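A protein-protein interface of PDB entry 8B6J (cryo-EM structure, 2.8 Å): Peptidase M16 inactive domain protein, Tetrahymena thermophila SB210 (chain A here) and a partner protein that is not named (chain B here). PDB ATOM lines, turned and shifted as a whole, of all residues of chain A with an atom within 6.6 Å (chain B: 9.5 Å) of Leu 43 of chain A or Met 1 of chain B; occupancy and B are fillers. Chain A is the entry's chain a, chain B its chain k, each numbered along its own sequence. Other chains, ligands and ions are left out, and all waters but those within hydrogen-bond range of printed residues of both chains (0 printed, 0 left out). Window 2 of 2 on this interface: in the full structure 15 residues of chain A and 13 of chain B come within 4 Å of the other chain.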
ATOM      1  N   SER A  39     -27.179 -18.136  -6.950  1.00  0.00           N
ATOM      2  CA  SER A  39     -26.239 -18.106  -8.060  1.00  0.00           C
ATOM      3  C   SER A  39     -24.990 -17.318  -7.688  1.00  0.00           C
ATOM      4  O   SER A  39     -25.024 -16.408  -6.856  1.00  0.00           O
ATOM      5  CB  SER A  39     -26.889 -17.487  -9.295  1.00  0.00           C
ATOM      6  OG  SER A  39     -25.938 -17.324 -10.332  1.00  0.00           O
ATOM      7  N   LYS A  40     -23.875 -17.681  -8.320  1.00  0.00           N
ATOM      8  CA  LYS A  40     -22.587 -17.031  -8.106  1.00  0.00           C
ATOM      9  C   LYS A  40     -22.091 -16.359  -9.381  1.00  0.00           C
ATOM     10  O   LYS A  40     -20.887 -16.181  -9.571  1.00  0.00           O
ATOM     11  CB  LYS A  40     -21.562 -18.042  -7.596  1.00  0.00           C
ATOM     12  CG  LYS A  40     -21.935 -18.669  -6.262  1.00  0.00           C
ATOM     13  CD  LYS A  40     -21.251 -20.010  -6.054  1.00  0.00           C
ATOM     14  CE  LYS A  40     -19.739 -19.882  -6.044  1.00  0.00           C
ATOM     15  NZ  LYS A  40     -19.080 -21.179  -5.722  1.00  0.00           N
ATOM     16  N   ALA A  41     -23.016 -15.981 -10.266  1.00  0.00           N
ATOM     17  CA  ALA A  41     -22.622 -15.373 -11.533  1.00  0.00           C
ATOM     18  C   ALA A  41     -22.151 -13.937 -11.342  1.00  0.00           C
ATOM     19  O   ALA A  41     -21.176 -13.510 -11.968  1.00  0.00           O
ATOM     20  CB  ALA A  41     -23.786 -15.426 -12.521  1.00  0.00           C
ATOM     21  N   ARG A  42     -22.835 -13.174 -10.486  1.00  0.00           N
ATOM     22  CA  ARG A  42     -22.472 -11.776 -10.285  1.00  0.00           C
ATOM     23  C   ARG A  42     -21.119 -11.620  -9.603  1.00  0.00           C
ATOM     24  O   ARG A  42     -20.516 -10.545  -9.692  1.00  0.00           O
ATOM     25  CB  ARG A  42     -23.554 -11.068  -9.470  1.00  0.00           C
ATOM     26  CG  ARG A  42     -24.915 -11.056 -10.146  1.00  0.00           C
ATOM     27  CD  ARG A  42     -25.975 -10.373  -9.295  1.00  0.00           C
ATOM     28  NE  ARG A  42     -25.725  -8.946  -9.131  1.00  0.00           N
ATOM     29  CZ  ARG A  42     -25.044  -8.407  -8.129  1.00  0.00           C
ATOM     30  NH1 ARG A  42     -24.514  -9.149  -7.170  1.00  0.00           N
ATOM     31  NH2 ARG A  42     -24.890  -7.086  -8.086  1.00  0.00           N
ATOM     32  N   LEU A  43     -20.627 -12.661  -8.930  1.00  0.00           N
ATOM     33  CA  LEU A  43     -19.323 -12.620  -8.268  1.00  0.00           C
ATOM     34  C   LEU A  43     -18.242 -12.763  -9.335  1.00  0.00           C
ATOM     35  O   LEU A  43     -17.631 -13.818  -9.518  1.00  0.00           O
ATOM     36  CB  LEU A  43     -19.221 -13.711  -7.212  1.00  0.00           C
ATOM     37  CG  LEU A  43     -19.906 -13.431  -5.873  1.00  0.00           C
ATOM     38  CD1 LEU A  43     -21.377 -13.109  -6.062  1.00  0.00           C
ATOM     39  CD2 LEU A  43     -19.735 -14.618  -4.940  1.00  0.00           C
ATOM     40  N   THR A  44     -17.999 -11.664 -10.047  1.00  0.00           N
ATOM     41  CA  THR A  44     -17.083 -11.648 -11.180  1.00  0.00           C
ATOM     42  C   THR A  44     -15.702 -11.119 -10.812  1.00  0.00           C
ATOM     43  O   THR A  44     -14.920 -10.780 -11.706  1.00  0.00           O
ATOM     44  CB  THR A  44     -17.671 -10.816 -12.320  1.00  0.00           C
ATOM     45  OG1 THR A  44     -17.911  -9.478 -11.866  1.00  0.00           O
ATOM     46  CG2 THR A  44     -18.976 -11.424 -12.810  1.00  0.00           C
ATOM     47  N   ASP A  45     -15.386 -11.034  -9.520  1.00  0.00           N
ATOM     48  CA  ASP A  45     -14.067 -10.600  -9.055  1.00  0.00           C
ATOM     49  C   ASP A  45     -13.562 -11.640  -8.060  1.00  0.00           C
ATOM     50  O   ASP A  45     -13.721 -11.480  -6.848  1.00  0.00           O
ATOM     51  CB  ASP A  45     -14.135  -9.205  -8.434  1.00  0.00           C
ATOM     52  CG  ASP A  45     -12.765  -8.635  -8.121  1.00  0.00           C
ATOM     53  OD1 ASP A  45     -11.837  -9.420  -7.839  1.00  0.00           O
ATOM     54  OD2 ASP A  45     -12.617  -7.396  -8.153  1.00  0.00           O
ATOM     55  N   PHE A  46     -12.940 -12.694  -8.586  1.00  0.00           N
ATOM     56  CA  PHE A  46     -12.298 -13.733  -7.785  1.00  0.00           C
ATOM     57  C   PHE A  46     -13.139 -14.099  -6.565  1.00  0.00           C
ATOM     58  O   PHE A  46     -12.667 -14.118  -5.428  1.00  0.00           O
ATOM     59  CB  PHE A  46     -10.897 -13.298  -7.368  1.00  0.00           C
ATOM     60  CG  PHE A  46     -10.013 -12.927  -8.524  1.00  0.00           C
ATOM     61  CD1 PHE A  46      -9.369 -13.904  -9.263  1.00  0.00           C
ATOM     62  CD2 PHE A  46      -9.828 -11.602  -8.873  1.00  0.00           C
ATOM     63  CE1 PHE A  46      -8.559 -13.566 -10.323  1.00  0.00           C
ATOM     64  CE2 PHE A  46      -9.019 -11.260  -9.934  1.00  0.00           C
ATOM     65  CZ  PHE A  46      -8.384 -12.243 -10.660  1.00  0.00           C
ATOM     66  N   GLY A  47     -14.412 -14.398  -6.816  1.00  0.00           N
ATOM     67  CA  GLY A  47     -15.308 -14.826  -5.764  1.00  0.00           C
ATOM     68  C   GLY A  47     -15.956 -13.712  -4.975  1.00  0.00           C
ATOM     69  O   GLY A  47     -16.612 -13.993  -3.967  1.00  0.00           O
ATOM     70  N   GLU A  48     -15.792 -12.460  -5.394  1.00  0.00           N
ATOM     71  CA  GLU A  48     -16.373 -11.325  -4.695  1.00  0.00           C
ATOM     72  C   GLU A  48     -16.953 -10.361  -5.721  1.00  0.00           C
ATOM     73  O   GLU A  48     -16.563 -10.361  -6.890  1.00  0.00           O
ATOM     74  CB  GLU A  48     -15.331 -10.616  -3.821  1.00  0.00           C
ATOM     75  CG  GLU A  48     -15.907  -9.617  -2.829  1.00  0.00           C
ATOM     76  CD  GLU A  48     -16.697 -10.278  -1.716  1.00  0.00           C
ATOM     77  OE1 GLU A  48     -16.816 -11.520  -1.721  1.00  0.00           O
ATOM     78  OE2 GLU A  48     -17.198  -9.553  -0.830  1.00  0.00           O
ATOM     79  N   LEU A  49     -17.902  -9.546  -5.272  1.00  0.00           N
ATOM     80  CA  LEU A  49     -18.486  -8.545  -6.147  1.00  0.00           C
ATOM     81  C   LEU A  49     -17.442  -7.486  -6.504  1.00  0.00           C
ATOM     82  O   LEU A  49     -16.524  -7.221  -5.725  1.00  0.00           O
ATOM     83  CB  LEU A  49     -19.682  -7.875  -5.476  1.00  0.00           C
ATOM     84  CG  LEU A  49     -20.869  -8.772  -5.129  1.00  0.00           C
ATOM     85  CD1 LEU A  49     -21.897  -7.997  -4.327  1.00  0.00           C
ATOM     86  CD2 LEU A  49     -21.496  -9.345  -6.387  1.00  0.00           C
ATOM     87  N   PRO A  50     -17.562  -6.861  -7.679  1.00  0.00           N
ATOM     88  CA  PRO A  50     -16.636  -5.775  -8.022  1.00  0.00           C
ATOM     89  C   PRO A  50     -16.836  -4.559  -7.129  1.00  0.00           C
ATOM     90  O   PRO A  50     -17.680  -4.577  -6.228  1.00  0.00           O
ATOM     91  CB  PRO A  50     -16.968  -5.473  -9.489  1.00  0.00           C
ATOM     92  CG  PRO A  50     -18.350  -5.975  -9.682  1.00  0.00           C
ATOM     93  CD  PRO A  50     -18.503  -7.151  -8.773  1.00  0.00           C
ATOM     94  N   MET B   1     -17.137 -15.350  -2.310  1.00  0.00           N
ATOM     95  CA  MET B   1     -16.346 -14.790  -1.181  1.00  0.00           C
ATOM     96  C   MET B   1     -14.866 -14.754  -1.532  1.00  0.00           C
ATOM     97  O   MET B   1     -14.394 -15.535  -2.356  1.00  0.00           O
ATOM     98  CB  MET B   1     -16.569 -15.611   0.088  1.00  0.00           C
ATOM     99  CG  MET B   1     -16.202 -17.075  -0.054  1.00  0.00           C
ATOM    100  SD  MET B   1     -16.639 -18.044   1.397  1.00  0.00           S
ATOM    101  CE  MET B   1     -18.421 -17.868   1.395  1.00  0.00           C
ATOM    102  N   TYR B   2     -14.140 -13.841  -0.894  1.00  0.00           N
ATOM    103  CA  TYR B   2     -12.727 -13.614  -1.169  1.00  0.00           C
ATOM    104  C   TYR B   2     -11.909 -14.349  -0.113  1.00  0.00           C
ATOM    105  O   TYR B   2     -11.901 -13.957   1.058  1.00  0.00           O
ATOM    106  CB  TYR B   2     -12.425 -12.117  -1.164  1.00  0.00           C
ATOM    107  CG  TYR B   2     -11.193 -11.713  -1.939  1.00  0.00           C
ATOM    108  CD1 TYR B   2     -11.158 -11.804  -3.322  1.00  0.00           C
ATOM    109  CD2 TYR B   2     -10.076 -11.209  -1.290  1.00  0.00           C
ATOM    110  CE1 TYR B   2     -10.039 -11.425  -4.033  1.00  0.00           C
ATOM    111  CE2 TYR B   2      -8.953 -10.829  -1.992  1.00  0.00           C
ATOM    112  CZ  TYR B   2      -8.939 -10.938  -3.363  1.00  0.00           C
ATOM    113  OH  TYR B   2      -7.820 -10.557  -4.066  1.00  0.00           O
ATOM    114  N   LEU B   3     -11.214 -15.407  -0.527  1.00  0.00           N
ATOM    115  CA  LEU B   3     -10.418 -16.243   0.372  1.00  0.00           C
ATOM    116  C   LEU B   3      -9.003 -16.341  -0.180  1.00  0.00           C
ATOM    117  O   LEU B   3      -8.566 -17.407  -0.630  1.00  0.00           O
ATOM    118  CB  LEU B   3     -11.033 -17.634   0.526  1.00  0.00           C
ATOM    119  CG  LEU B   3     -12.483 -17.708   1.006  1.00  0.00           C
ATOM    120  CD1 LEU B   3     -12.919 -19.155   1.138  1.00  0.00           C
ATOM    121  CD2 LEU B   3     -12.659 -16.978   2.322  1.00  0.00           C
ATOM    122  N   PRO B   4      -8.255 -15.243  -0.156  1.00  0.00           N
ATOM    123  CA  PRO B   4      -6.891 -15.273  -0.690  1.00  0.00           C
ATOM    124  C   PRO B   4      -5.989 -16.180   0.130  1.00  0.00           C
ATOM    125  O   PRO B   4      -6.137 -16.312   1.347  1.00  0.00           O
ATOM    126  CB  PRO B   4      -6.445 -13.810  -0.603  1.00  0.00           C
ATOM    127  CG  PRO B   4      -7.265 -13.232   0.487  1.00  0.00           C
ATOM    128  CD  PRO B   4      -8.587 -13.940   0.441  1.00  0.00           C
ATOM    129  N   LYS B   8      -0.218 -15.458  -0.662  1.00  0.00           N
ATOM    130  CA  LYS B   8      -0.406 -14.204  -1.381  1.00  0.00           C
ATOM    131  C   LYS B   8      -0.393 -13.014  -0.432  1.00  0.00           C
ATOM    132  O   LYS B   8       0.168 -11.963  -0.759  1.00  0.00           O
ATOM    133  CB  LYS B   8      -1.712 -14.243  -2.171  1.00  0.00           C
ATOM    134  CG  LYS B   8      -1.946 -12.998  -3.004  1.00  0.00           C
ATOM    135  CD  LYS B   8      -3.165 -13.125  -3.888  1.00  0.00           C
ATOM    136  CE  LYS B   8      -4.435 -13.134  -3.070  1.00  0.00           C
ATOM    137  NZ  LYS B   8      -5.627 -12.973  -3.936  1.00  0.00           N
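Among the printed residues, merely in contact across the chains: Glu 48 of chain A with Met 1 of chain B (3.3 Å), Phe 46 of chain A with Tyr 2 of chain B (3.5 Å), Glu 48 of chain A with Tyr 2 of chain B (3.6 Å), Leu 43 of chain A with Met 1 of chain B (3.8 Å), Phe 46 of chain A with Met 1 of chain B (3.8 Å) and Gly 47 of chain A with Tyr 2 of chain B (3.9 Å).
Leu 43 of chain A touches just one residue of chain B: Met 1.
No residue of chain B comes within 4 Å of Thr 44 of chain A.
Of the printed residues of chain B, Phe 46 of chain A touches Met 1 and Tyr 2.
Gly 47 of chain A touches just these residues of chain B: Met 1 (2.2 Å) and Tyr 2 (3.9 Å).
Of chain B, only Met 1 (3.3 Å) and Tyr 2 (3.6 Å) come within 4 Å of Glu 48 of chain A.
Leu 49 of chain A touches none of the printed residues of chain B.
Met 1 of chain B touches four residues of chain A.
Of the printed residues of chain A, Tyr 2 of chain B touches Phe 46 (3.5 Å), Gly 47 (3.9 Å) and Glu 48 (3.6 Å).
The nearest residue of chain A that does not touch Met 1 of chain B is Asp 45 of chain A (6.1 Å).
The nearest printed residue of chain A that does not touch Tyr 2 of chain B is Asp 45 of chain A (4.4 Å).
Of the 5 printed residues of chain B, 2 touch a printed residue of chain A.
Printed residues of chain B that touch a printed residue of chain A: Met 1 and Tyr 2.
Hydrophobic or aromatic side chains of chain B within 4 Å of the printed part of chain A: Tyr 2.
Of the 12 printed residues of chain A, 4 touch a printed residue of chain B.
Among the printed residues, 7 pairs touch across the chains.
Among the printed residues, no Asp or Glu carboxylate lies within 4 Å of a Lys or Arg side-chain nitrogen of the other chain.
The side-chain amino group of Lys 8 of chain B sits at hydrogen-bond distance from the side-chain hydroxyl of Tyr 2 of chain B (3.3 Å).
O of Gly 47 of chain A lies close to N of Met 1 of chain B.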
